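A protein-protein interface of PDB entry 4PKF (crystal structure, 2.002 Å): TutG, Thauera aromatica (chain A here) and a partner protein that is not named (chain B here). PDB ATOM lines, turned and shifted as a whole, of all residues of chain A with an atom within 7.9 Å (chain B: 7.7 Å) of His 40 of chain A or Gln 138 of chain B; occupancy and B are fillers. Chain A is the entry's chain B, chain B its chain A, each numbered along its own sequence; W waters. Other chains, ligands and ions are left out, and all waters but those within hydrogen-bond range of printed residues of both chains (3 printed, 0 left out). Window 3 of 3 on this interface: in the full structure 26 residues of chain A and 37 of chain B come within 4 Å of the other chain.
The side-chain amide nitrogen of Gln 138 of chain B sits at hydrogen-bond distance from a ring nitrogen (NE2) of His 40 of chain A. The guanidinium group (NH2) of Arg 142 of chain B lies within hydrogen-bond range of the backbone carbonyl oxygen (O) of Pro 39 of chain A (3.3 Å). The guanidinium group (NE) of Arg 27 of chain A sits close to the guanidinium group (NH2) of Arg 142 of chain B (3.3 Å). The guanidinium group (NH2) of Arg 142 of chain B is in salt-bridge range of the side-chain carboxylate (OE2) of Glu 63 of chain A (3.8 Å). O of Thr 37 of chain A sits close to SD of Met 135 of chain B, 3.8 Å away.
The backbone NH (N) of His 40 of chain A sits at hydrogen-bond distance from the side-chain carboxylate (OD1) of Asp 38 of chain A. N of Asp 38 of chain A lies within hydrogen-bond range of OD1 of Asp 35 of chain A (2.9 Å). OD1 of Asp 35 of chain A sits at hydrogen-bond distance from N of Thr 37 of chain A. The side-chain hydroxyl (OG) of Ser 133 of chain B sits close to the backbone NH (N) of Met 135 of chain B (3.4 Å). OD1 of Asp 61 of chain A is in hydrogen-bond range of N of Glu 63 of chain A. The side-chain carboxylate (OD2) of Asp 38 of chain A is in salt-bridge range of the guanidinium group (NE) of Arg 41 of chain A, 3.7 Å away.
Pro 34 of chain A touches Asp 139 of chain B (CB to OD1, 3.999 Å). SD of Met 135 of chain B touches CB of Asp 38 of chain A (3.8 Å). Pro 39 of chain A touches Met 135 of chain B. CG of Pro 39 of chain A touches OE1 of Gln 138 of chain B (3.6 Å). Pro 39 of chain A touches Asp 139 of chain B (CG to N, 3.7 Å). NH1 of Arg 142 of chain B touches CD2 of His 40 of chain A, 3.8 Å away.
Printed residues of chain B within 4 Å of Arg 27 of chain A: Arg 142 (3.3 Å). Asp 35 of chain A touches none of the printed residues of chain B. Printed residues of chain B within 4 Å of Asp 38 of chain A: Met 135. Printed residues of chain B within 4 Å of Pro 39 of chain A: Met 135, Gln 138, Asp 139 and Arg 142. His 40 of chain A touches just these residues of chain B: Gln 138 (2.8 Å) and Arg 142 (3.8 Å). Gln 138 of chain B touches two residues of chain A. Printed residues of chain A within 4 Å of Arg 142 of chain B: Arg 27 (3.3 Å), Pro 39 (3.3 Å), His 40 (3.8 Å) and Glu 63 (3.8 Å). The nearest residue of chain A that does not touch Gln 138 of chain B is Asp 38 of chain A (4.9 Å). The nearest printed residue of chain A that does not touch Arg 142 of chain B is Val 62 of chain A (4.3 Å).
Of the 17 printed residues of chain B, 4 touch a printed residue of chain A. Among the printed residues, Asp or Glu carboxylates within 4 Å of a Lys or Arg side-chain nitrogen of the other chain: Glu 63 of chain A with Arg 142 of chain B (3.8 Å).
Water W3 lies within hydrogen-bond range of the side-chain carboxylate of Asp 139 of chain B (2.6 Å) and the backbone carbonyl oxygen of Asp 35 of chain A (2.9 Å). Water W2 lies within hydrogen-bond range of OD1 of Asp 38 of chain A (2.7 Å), OE1 of Gln 138 of chain B (2.8 Å) and ND1 of His 40 of chain A (3.4 Å). Water W1 bridges the backbone carbonyl oxygen of Pro 39 of chain A (2.9 Å) and the guanidinium group of Arg 142 of chain B (3.0 Å).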
ATOM      1  N   ARG A  27      -3.410 -20.531  -3.288  1.00  0.00           N
ATOM      2  CA  ARG A  27      -2.128 -19.836  -3.189  1.00  0.00           C
ATOM      3  C   ARG A  27      -2.044 -18.880  -1.995  1.00  0.00           C
ATOM      4  O   ARG A  27      -0.964 -18.683  -1.419  1.00  0.00           O
ATOM      5  CB  ARG A  27      -1.831 -19.055  -4.464  1.00  0.00           C
ATOM      6  CG  ARG A  27      -0.396 -18.603  -4.518  1.00  0.00           C
ATOM      7  CD  ARG A  27      -0.022 -18.075  -5.866  1.00  0.00           C
ATOM      8  NE  ARG A  27       1.325 -17.517  -5.822  1.00  0.00           N
ATOM      9  CZ  ARG A  27       1.855 -16.803  -6.802  1.00  0.00           C
ATOM     10  NH1 ARG A  27       1.152 -16.563  -7.903  1.00  0.00           N
ATOM     11  NH2 ARG A  27       3.079 -16.325  -6.679  1.00  0.00           N
ATOM     12  N   GLN A  32      -2.168 -23.916   2.701  1.00  0.00           N
ATOM     13  CA  GLN A  32      -1.369 -24.285   1.521  1.00  0.00           C
ATOM     14  C   GLN A  32       0.122 -24.047   1.747  1.00  0.00           C
ATOM     15  O   GLN A  32       0.506 -23.060   2.365  1.00  0.00           O
ATOM     16  CB  GLN A  32      -1.806 -23.490   0.285  1.00  0.00           C
ATOM     17  CG  GLN A  32      -1.259 -23.978  -1.063  1.00  0.00           C
ATOM     18  CD  GLN A  32       0.100 -23.357  -1.484  1.00  0.00           C
ATOM     19  OE1 GLN A  32       0.715 -23.834  -2.428  1.00  0.00           O
ATOM     20  NE2 GLN A  32       0.546 -22.303  -0.803  1.00  0.00           N
ATOM     21  N   PRO A  34       3.702 -24.602  -1.000  1.00  0.00           N
ATOM     22  CA  PRO A  34       3.972 -25.021  -2.387  1.00  0.00           C
ATOM     23  C   PRO A  34       4.491 -26.471  -2.486  1.00  0.00           C
ATOM     24  O   PRO A  34       5.105 -26.993  -1.564  1.00  0.00           O
ATOM     25  CB  PRO A  34       5.049 -24.022  -2.855  1.00  0.00           C
ATOM     26  CG  PRO A  34       4.866 -22.816  -1.983  1.00  0.00           C
ATOM     27  CD  PRO A  34       4.416 -23.360  -0.640  1.00  0.00           C
ATOM     28  N   ASP A  35       4.192 -27.112  -3.607  1.00  0.00           N
ATOM     29  CA  ASP A  35       4.727 -28.419  -3.984  1.00  0.00           C
ATOM     30  C   ASP A  35       6.276 -28.451  -3.903  1.00  0.00           C
ATOM     31  O   ASP A  35       6.934 -27.448  -4.162  1.00  0.00           O
ATOM     32  CB  ASP A  35       4.221 -28.716  -5.407  1.00  0.00           C
ATOM     33  CG  ASP A  35       4.699 -30.031  -5.977  1.00  0.00           C
ATOM     34  OD1 ASP A  35       5.827 -30.073  -6.498  1.00  0.00           O
ATOM     35  OD2 ASP A  35       3.920 -31.017  -5.985  1.00  0.00           O
ATOM     36  N   THR A  37       8.568 -29.747  -5.767  1.00  0.00           N
ATOM     37  CA  THR A  37       9.307 -29.680  -7.038  1.00  0.00           C
ATOM     38  C   THR A  37       8.870 -28.520  -7.935  1.00  0.00           C
ATOM     39  O   THR A  37       9.689 -27.803  -8.521  1.00  0.00           O
ATOM     40  CB  THR A  37       9.086 -30.969  -7.880  1.00  0.00           C
ATOM     41  OG1 THR A  37       9.350 -32.128  -7.090  1.00  0.00           O
ATOM     42  CG2 THR A  37       9.979 -30.968  -9.140  1.00  0.00           C
ATOM     43  N   ASP A  38       7.552 -28.405  -8.104  1.00  0.00           N
ATOM     44  CA  ASP A  38       6.954 -27.466  -9.061  1.00  0.00           C
ATOM     45  C   ASP A  38       6.091 -26.407  -8.359  1.00  0.00           C
ATOM     46  O   ASP A  38       4.994 -26.716  -7.851  1.00  0.00           O
ATOM     47  CB  ASP A  38       6.121 -28.257 -10.082  1.00  0.00           C
ATOM     48  CG  ASP A  38       5.478 -27.374 -11.159  1.00  0.00           C
ATOM     49  OD1 ASP A  38       5.519 -26.140 -11.089  1.00  0.00           O
ATOM     50  OD2 ASP A  38       4.893 -27.940 -12.072  1.00  0.00           O
ATOM     51  N   PRO A  39       6.563 -25.146  -8.349  1.00  0.00           N
ATOM     52  CA  PRO A  39       5.851 -24.120  -7.566  1.00  0.00           C
ATOM     53  C   PRO A  39       4.478 -23.736  -8.151  1.00  0.00           C
ATOM     54  O   PRO A  39       3.757 -22.967  -7.505  1.00  0.00           O
ATOM     55  CB  PRO A  39       6.809 -22.930  -7.592  1.00  0.00           C
ATOM     56  CG  PRO A  39       7.591 -23.139  -8.892  1.00  0.00           C
ATOM     57  CD  PRO A  39       7.777 -24.611  -9.001  1.00  0.00           C
ATOM     58  N   HIS A  40       4.127 -24.270  -9.321  1.00  0.00           N
ATOM     59  CA  HIS A  40       2.776 -24.127  -9.865  1.00  0.00           C
ATOM     60  C   HIS A  40       1.785 -25.004  -9.124  1.00  0.00           C
ATOM     61  O   HIS A  40       0.589 -24.758  -9.166  1.00  0.00           O
ATOM     62  CB  HIS A  40       2.751 -24.479 -11.361  1.00  0.00           C
ATOM     63  CG  HIS A  40       3.340 -23.413 -12.234  1.00  0.00           C
ATOM     64  ND1 HIS A  40       3.601 -23.604 -13.576  1.00  0.00           N
ATOM     65  CD2 HIS A  40       3.716 -22.141 -11.954  1.00  0.00           C
ATOM     66  CE1 HIS A  40       4.113 -22.496 -14.083  1.00  0.00           C
ATOM     67  NE2 HIS A  40       4.187 -21.591 -13.122  1.00  0.00           N
ATOM     68  N   ARG A  41       2.291 -26.043  -8.472  1.00  0.00           N
ATOM     69  CA  ARG A  41       1.471 -26.957  -7.706  1.00  0.00           C
ATOM     70  C   ARG A  41       1.520 -26.632  -6.221  1.00  0.00           C
ATOM     71  O   ARG A  41       2.375 -25.881  -5.768  1.00  0.00           O
ATOM     72  CB  ARG A  41       1.922 -28.401  -7.913  1.00  0.00           C
ATOM     73  CG  ARG A  41       2.346 -28.727  -9.338  1.00  0.00           C
ATOM     74  CD  ARG A  41       1.188 -28.765 -10.263  1.00  0.00           C
ATOM     75  NE  ARG A  41       1.559 -29.454 -11.498  1.00  0.00           N
ATOM     76  CZ  ARG A  41       0.697 -29.846 -12.430  1.00  0.00           C
ATOM     77  NH1 ARG A  41       1.133 -30.464 -13.522  1.00  0.00           N
ATOM     78  NH2 ARG A  41      -0.592 -29.612 -12.280  1.00  0.00           N
ATOM     79  N   GLY A  42       0.603 -27.217  -5.462  1.00  0.00           N
ATOM     80  CA  GLY A  42       0.553 -26.950  -4.038  1.00  0.00           C
ATOM     81  C   GLY A  42       0.245 -28.155  -3.169  1.00  0.00           C
ATOM     82  O   GLY A  42      -0.105 -29.208  -3.673  1.00  0.00           O
ATOM     83  N   TRP A  58      -2.833 -33.070  -2.668  1.00  0.00           N
ATOM     84  CA  TRP A  58      -2.059 -32.417  -3.724  1.00  0.00           C
ATOM     85  C   TRP A  58      -2.918 -31.438  -4.537  1.00  0.00           C
ATOM     86  O   TRP A  58      -4.051 -31.759  -4.902  1.00  0.00           O
ATOM     87  CB  TRP A  58      -1.426 -33.477  -4.651  1.00  0.00           C
ATOM     88  CG  TRP A  58      -0.485 -32.908  -5.670  1.00  0.00           C
ATOM     89  CD1 TRP A  58       0.701 -32.229  -5.428  1.00  0.00           C
ATOM     90  CD2 TRP A  58      -0.630 -32.948  -7.094  1.00  0.00           C
ATOM     91  NE1 TRP A  58       1.284 -31.874  -6.603  1.00  0.00           N
ATOM     92  CE2 TRP A  58       0.500 -32.301  -7.644  1.00  0.00           C
ATOM     93  CE3 TRP A  58      -1.577 -33.509  -7.960  1.00  0.00           C
ATOM     94  CZ2 TRP A  58       0.696 -32.182  -9.025  1.00  0.00           C
ATOM     95  CZ3 TRP A  58      -1.402 -33.379  -9.309  1.00  0.00           C
ATOM     96  CH2 TRP A  58      -0.260 -32.727  -9.843  1.00  0.00           C
ATOM     97  N   LEU A  59      -2.384 -30.253  -4.802  1.00  0.00           N
ATOM     98  CA  LEU A  59      -3.121 -29.242  -5.546  1.00  0.00           C
ATOM     99  C   LEU A  59      -2.488 -29.033  -6.933  1.00  0.00           C
ATOM    100  O   LEU A  59      -1.350 -28.544  -7.017  1.00  0.00           O
ATOM    101  CB  LEU A  59      -3.140 -27.920  -4.762  1.00  0.00           C
ATOM    102  CG  LEU A  59      -3.675 -27.931  -3.314  1.00  0.00           C
ATOM    103  CD1 LEU A  59      -3.427 -26.584  -2.655  1.00  0.00           C
ATOM    104  CD2 LEU A  59      -5.184 -28.297  -3.296  1.00  0.00           C
ATOM    105  N   ARG A  60      -3.229 -29.412  -7.985  1.00  0.00           N
ATOM    106  CA  ARG A  60      -2.810 -29.285  -9.390  1.00  0.00           C
ATOM    107  C   ARG A  60      -2.624 -27.856  -9.800  1.00  0.00           C
ATOM    108  O   ARG A  60      -1.807 -27.526 -10.667  1.00  0.00           O
ATOM    109  CB  ARG A  60      -3.842 -29.912 -10.323  1.00  0.00           C
ATOM    110  CG  ARG A  60      -3.904 -31.392 -10.204  1.00  0.00           C
ATOM    111  CD  ARG A  60      -5.190 -31.990 -10.767  1.00  0.00           C
ATOM    112  NE  ARG A  60      -5.017 -33.435 -10.864  1.00  0.00           N
ATOM    113  CZ  ARG A  60      -5.068 -34.277  -9.830  1.00  0.00           C
ATOM    114  NH1 ARG A  60      -5.315 -33.838  -8.592  1.00  0.00           N
ATOM    115  NH2 ARG A  60      -4.881 -35.573 -10.044  1.00  0.00           N
ATOM    116  N   ASP A  61      -3.425 -27.001  -9.189  1.00  0.00           N
ATOM    117  CA  ASP A  61      -3.408 -25.597  -9.536  1.00  0.00           C
ATOM    118  C   ASP A  61      -3.829 -24.757  -8.354  1.00  0.00           C
ATOM    119  O   ASP A  61      -4.902 -24.959  -7.808  1.00  0.00           O
ATOM    120  CB  ASP A  61      -4.341 -25.324 -10.714  1.00  0.00           C
ATOM    121  CG  ASP A  61      -4.762 -23.885 -10.765  1.00  0.00           C
ATOM    122  OD1 ASP A  61      -3.953 -23.034 -11.199  1.00  0.00           O
ATOM    123  OD2 ASP A  61      -5.880 -23.608 -10.305  1.00  0.00           O
ATOM    124  N   VAL A  62      -2.999 -23.809  -7.964  1.00  0.00           N
ATOM    125  CA  VAL A  62      -3.285 -23.023  -6.778  1.00  0.00           C
ATOM    126  C   VAL A  62      -3.877 -21.639  -7.063  1.00  0.00           C
ATOM    127  O   VAL A  62      -4.098 -20.864  -6.137  1.00  0.00           O
ATOM    128  CB  VAL A  62      -2.010 -22.861  -5.938  1.00  0.00           C
ATOM    129  CG1 VAL A  62      -1.580 -24.226  -5.388  1.00  0.00           C
ATOM    130  CG2 VAL A  62      -0.906 -22.253  -6.794  1.00  0.00           C
ATOM    131  N   GLU A  63      -4.131 -21.323  -8.329  1.00  0.00           N
ATOM    132  CA  GLU A  63      -4.732 -20.034  -8.680  1.00  0.00           C
ATOM    133  C   GLU A  63      -6.224 -20.140  -8.879  1.00  0.00           C
ATOM    134  O   GLU A  63      -6.941 -19.163  -8.704  1.00  0.00           O
ATOM    135  CB  GLU A  63      -4.115 -19.457  -9.956  1.00  0.00           C
ATOM    136  CG  GLU A  63      -2.615 -19.457  -9.996  1.00  0.00           C
ATOM    137  CD  GLU A  63      -1.976 -18.393  -9.108  1.00  0.00           C
ATOM    138  OE1 GLU A  63      -2.705 -17.555  -8.525  1.00  0.00           O
ATOM    139  OE2 GLU A  63      -0.727 -18.406  -9.007  1.00  0.00           O
ATOM    140  N   LEU B 128      22.210 -18.875  -6.014  1.00  0.00           N
ATOM    141  CA  LEU B 128      21.265 -19.737  -6.722  1.00  0.00           C
ATOM    142  C   LEU B 128      21.895 -20.307  -7.999  1.00  0.00           C
ATOM    143  O   LEU B 128      23.010 -19.926  -8.380  1.00  0.00           O
ATOM    144  CB  LEU B 128      20.003 -18.977  -7.074  1.00  0.00           C
ATOM    145  CG  LEU B 128      19.195 -18.572  -5.834  1.00  0.00           C
ATOM    146  CD1 LEU B 128      17.892 -17.900  -6.264  1.00  0.00           C
ATOM    147  CD2 LEU B 128      18.895 -19.796  -4.924  1.00  0.00           C
ATOM    148  N   SER B 133      17.944 -26.324 -12.236  1.00  0.00           N
ATOM    149  CA  SER B 133      16.491 -26.470 -12.284  1.00  0.00           C
ATOM    150  C   SER B 133      15.783 -25.131 -12.434  1.00  0.00           C
ATOM    151  O   SER B 133      15.874 -24.302 -11.538  1.00  0.00           O
ATOM    152  CB  SER B 133      15.984 -27.141 -11.001  1.00  0.00           C
ATOM    153  OG  SER B 133      14.578 -27.003 -10.891  1.00  0.00           O
ATOM    154  N   HIS B 134      15.088 -24.902 -13.550  1.00  0.00           N
ATOM    155  CA  HIS B 134      14.344 -23.653 -13.708  1.00  0.00           C
ATOM    156  C   HIS B 134      13.175 -23.584 -12.729  1.00  0.00           C
ATOM    157  O   HIS B 134      12.817 -22.497 -12.258  1.00  0.00           O
ATOM    158  CB  HIS B 134      13.840 -23.464 -15.159  1.00  0.00           C
ATOM    159  CG  HIS B 134      13.168 -24.671 -15.734  1.00  0.00           C
ATOM    160  ND1 HIS B 134      13.855 -25.637 -16.436  1.00  0.00           N
ATOM    161  CD2 HIS B 134      11.867 -25.058 -15.728  1.00  0.00           C
ATOM    162  CE1 HIS B 134      13.006 -26.563 -16.853  1.00  0.00           C
ATOM    163  NE2 HIS B 134      11.797 -26.245 -16.421  1.00  0.00           N
ATOM    164  N   MET B 135      12.599 -24.734 -12.393  1.00  0.00           N
ATOM    165  CA  MET B 135      11.543 -24.756 -11.387  1.00  0.00           C
ATOM    166  C   MET B 135      12.015 -24.308 -10.003  1.00  0.00           C
ATOM    167  O   MET B 135      11.299 -23.596  -9.296  1.00  0.00           O
ATOM    168  CB  MET B 135      10.921 -26.156 -11.280  1.00  0.00           C
ATOM    169  CG  MET B 135      10.013 -26.487 -12.469  1.00  0.00           C
ATOM    170  SD  MET B 135       9.228 -28.102 -12.234  1.00  0.00           S
ATOM    171  CE  MET B 135       8.506 -28.403 -13.864  1.00  0.00           C
ATOM    172  N   ALA B 136      13.203 -24.739  -9.600  1.00  0.00           N
ATOM    173  CA  ALA B 136      13.703 -24.362  -8.280  1.00  0.00           C
ATOM    174  C   ALA B 136      13.897 -22.858  -8.214  1.00  0.00           C
ATOM    175  O   ALA B 136      13.625 -22.241  -7.200  1.00  0.00           O
ATOM    176  CB  ALA B 136      15.026 -25.097  -7.957  1.00  0.00           C
ATOM    177  N   VAL B 137      14.388 -22.265  -9.292  1.00  0.00           N
ATOM    178  CA  VAL B 137      14.594 -20.832  -9.288  1.00  0.00           C
ATOM    179  C   VAL B 137      13.244 -20.135  -9.232  1.00  0.00           C
ATOM    180  O   VAL B 137      13.066 -19.186  -8.471  1.00  0.00           O
ATOM    181  CB  VAL B 137      15.388 -20.364 -10.511  1.00  0.00           C
ATOM    182  CG1 VAL B 137      15.429 -18.854 -10.554  1.00  0.00           C
ATOM    183  CG2 VAL B 137      16.794 -20.929 -10.434  1.00  0.00           C
ATOM    184  N   GLN B 138      12.279 -20.622 -10.025  1.00  0.00           N
ATOM    185  CA  GLN B 138      10.957 -20.038 -10.016  1.00  0.00           C
ATOM    186  C   GLN B 138      10.334 -20.087  -8.623  1.00  0.00           C
ATOM    187  O   GLN B 138       9.682 -19.133  -8.183  1.00  0.00           O
ATOM    188  CB  GLN B 138      10.036 -20.749 -11.039  1.00  0.00           C
ATOM    189  CG  GLN B 138       8.668 -20.088 -11.152  1.00  0.00           C
ATOM    190  CD  GLN B 138       7.643 -20.952 -11.890  1.00  0.00           C
ATOM    191  OE1 GLN B 138       7.922 -22.096 -12.300  1.00  0.00           O
ATOM    192  NE2 GLN B 138       6.438 -20.409 -12.048  1.00  0.00           N
ATOM    193  N   ASP B 139      10.535 -21.194  -7.920  1.00  0.00           N
ATOM    194  CA  ASP B 139      10.063 -21.291  -6.559  1.00  0.00           C
ATOM    195  C   ASP B 139      10.697 -20.198  -5.675  1.00  0.00           C
ATOM    196  O   ASP B 139       9.999 -19.578  -4.866  1.00  0.00           O
ATOM    197  CB  ASP B 139      10.345 -22.695  -6.009  1.00  0.00           C
ATOM    198  CG  ASP B 139       9.856 -22.870  -4.572  1.00  0.00           C
ATOM    199  OD1 ASP B 139       8.695 -23.335  -4.347  1.00  0.00           O
ATOM    200  OD2 ASP B 139      10.652 -22.552  -3.661  1.00  0.00           O
ATOM    201  N   TYR B 140      12.002 -19.932  -5.837  1.00  0.00           N
ATOM    202  CA  TYR B 140      12.662 -18.843  -5.088  1.00  0.00           C
ATOM    203  C   TYR B 140      12.071 -17.468  -5.427  1.00  0.00           C
ATOM    204  O   TYR B 140      11.866 -16.627  -4.552  1.00  0.00           O
ATOM    205  CB  TYR B 140      14.184 -18.848  -5.341  1.00  0.00           C
ATOM    206  CG  TYR B 140      14.962 -19.718  -4.369  1.00  0.00           C
ATOM    207  CD1 TYR B 140      15.174 -19.291  -3.047  1.00  0.00           C
ATOM    208  CD2 TYR B 140      15.498 -20.961  -4.756  1.00  0.00           C
ATOM    209  CE1 TYR B 140      15.886 -20.065  -2.130  1.00  0.00           C
ATOM    210  CE2 TYR B 140      16.237 -21.743  -3.851  1.00  0.00           C
ATOM    211  CZ  TYR B 140      16.433 -21.281  -2.538  1.00  0.00           C
ATOM    212  OH  TYR B 140      17.107 -22.022  -1.580  1.00  0.00           O
ATOM    213  N   LEU B 141      11.711 -17.279  -6.680  1.00  0.00           N
ATOM    214  CA  LEU B 141      11.174 -16.010  -7.119  1.00  0.00           C
ATOM    215  C   LEU B 141       9.816 -15.765  -6.525  1.00  0.00           C
ATOM    216  O   LEU B 141       9.405 -14.620  -6.377  1.00  0.00           O
ATOM    217  CB  LEU B 141      11.070 -15.963  -8.644  1.00  0.00           C
ATOM    218  CG  LEU B 141      12.360 -15.897  -9.453  1.00  0.00           C
ATOM    219  CD1 LEU B 141      12.025 -15.997 -10.965  1.00  0.00           C
ATOM    220  CD2 LEU B 141      13.109 -14.630  -9.164  1.00  0.00           C
ATOM    221  N   ARG B 142       9.105 -16.844  -6.208  1.00  0.00           N
ATOM    222  CA  ARG B 142       7.798 -16.746  -5.584  1.00  0.00           C
ATOM    223  C   ARG B 142       7.857 -16.690  -4.046  1.00  0.00           C
ATOM    224  O   ARG B 142       6.826 -16.654  -3.398  1.00  0.00           O
ATOM    225  CB  ARG B 142       6.937 -17.933  -6.018  1.00  0.00           C
ATOM    226  CG  ARG B 142       6.600 -17.873  -7.480  1.00  0.00           C
ATOM    227  CD  ARG B 142       6.146 -19.207  -7.988  1.00  0.00           C
ATOM    228  NE  ARG B 142       4.807 -19.554  -7.525  1.00  0.00           N
ATOM    229  CZ  ARG B 142       3.728 -19.539  -8.311  1.00  0.00           C
ATOM    230  NH1 ARG B 142       3.845 -19.172  -9.591  1.00  0.00           N
ATOM    231  NH2 ARG B 142       2.540 -19.887  -7.818  1.00  0.00           N
ATOM    232  N   SER B 143       9.060 -16.692  -3.473  1.00  0.00           N
ATOM    233  CA  SER B 143       9.218 -16.718  -2.020  1.00  0.00           C
ATOM    234  C   SER B 143       9.549 -15.351  -1.428  1.00  0.00           C
ATOM    235  O   SER B 143       9.919 -14.418  -2.144  1.00  0.00           O
ATOM    236  CB  SER B 143      10.319 -17.700  -1.640  1.00  0.00           C
ATOM    237  OG  SER B 143      11.590 -17.058  -1.821  1.00  0.00           O
ATOM    238  N   SER B 146      13.327 -14.150  -2.219  1.00  0.00           N
ATOM    239  CA  SER B 146      13.701 -14.064  -3.620  1.00  0.00           C
ATOM    240  C   SER B 146      15.005 -13.300  -3.793  1.00  0.00           C
ATOM    241  O   SER B 146      15.292 -12.364  -3.035  1.00  0.00           O
ATOM    242  CB  SER B 146      12.599 -13.375  -4.447  1.00  0.00           C
ATOM    243  OG  SER B 146      13.108 -12.979  -5.727  1.00  0.00           O
ATOM    244  N   ALA B 153      16.270 -11.125 -11.902  1.00  0.00           N
ATOM    245  CA  ALA B 153      16.333 -12.537 -11.561  1.00  0.00           C
ATOM    246  C   ALA B 153      15.369 -13.338 -12.446  1.00  0.00           C
ATOM    247  O   ALA B 153      15.687 -14.434 -12.901  1.00  0.00           O
ATOM    248  CB  ALA B 153      15.993 -12.737 -10.060  1.00  0.00           C
ATOM    249  N   ASN B 157      16.214 -16.257 -15.177  1.00  0.00           N
ATOM    250  CA  ASN B 157      15.707 -17.626 -15.199  1.00  0.00           C
ATOM    251  C   ASN B 157      15.109 -17.963 -16.565  1.00  0.00           C
ATOM    252  O   ASN B 157      15.157 -19.118 -17.010  1.00  0.00           O
ATOM    253  CB  ASN B 157      14.647 -17.866 -14.112  1.00  0.00           C
ATOM    254  CG  ASN B 157      14.472 -19.350 -13.800  1.00  0.00           C
ATOM    255  OD1 ASN B 157      15.434 -20.126 -13.865  1.00  0.00           O
ATOM    256  ND2 ASN B 157      13.261 -19.742 -13.433  1.00  0.00           N
ATOM    257  N   GLU B 158      14.527 -16.963 -17.222  1.00  0.00           N
ATOM    258  CA  GLU B 158      13.944 -17.208 -18.545  1.00  0.00           C
ATOM    259  C   GLU B 158      15.061 -17.444 -19.553  1.00  0.00           C
ATOM    260  O   GLU B 158      14.934 -18.254 -20.461  1.00  0.00           O
ATOM    261  CB  GLU B 158      13.051 -16.048 -18.968  1.00  0.00           C
ATOM    262  CG  GLU B 158      11.734 -16.012 -18.205  1.00  0.00           C
ATOM    263  CD  GLU B 158      10.893 -17.296 -18.416  1.00  0.00           C
ATOM    264  OE1 GLU B 158      10.743 -17.745 -19.587  1.00  0.00           O
ATOM    265  OE2 GLU B 158      10.398 -17.864 -17.405  1.00  0.00           O
ATOM    266  N   LYS B 161      16.331 -21.160 -18.960  1.00  0.00           N
ATOM    267  CA  LYS B 161      15.387 -22.288 -18.997  1.00  0.00           C
ATOM    268  C   LYS B 161      15.655 -23.285 -20.155  1.00  0.00           C
ATOM    269  O   LYS B 161      15.760 -24.479 -19.895  1.00  0.00           O
ATOM    270  CB  LYS B 161      13.933 -21.794 -19.033  1.00  0.00           C
ATOM    271  CG  LYS B 161      12.892 -22.942 -19.014  1.00  0.00           C
ATOM    272  CD  LYS B 161      11.459 -22.444 -18.877  1.00  0.00           C
ATOM    273  CE  LYS B 161      10.470 -23.585 -19.276  1.00  0.00           C
ATOM    274  NZ  LYS B 161       9.063 -23.188 -19.005  1.00  0.00           N
HETATM  275  O   HOH W   1       4.136 -21.289  -5.170  1.00  0.00           O
HETATM  276  O   HOH W   2       6.749 -24.578 -12.881  1.00  0.00           O
HETATM  277  O   HOH W   3       8.619 -25.630  -5.668  1.00  0.00           O
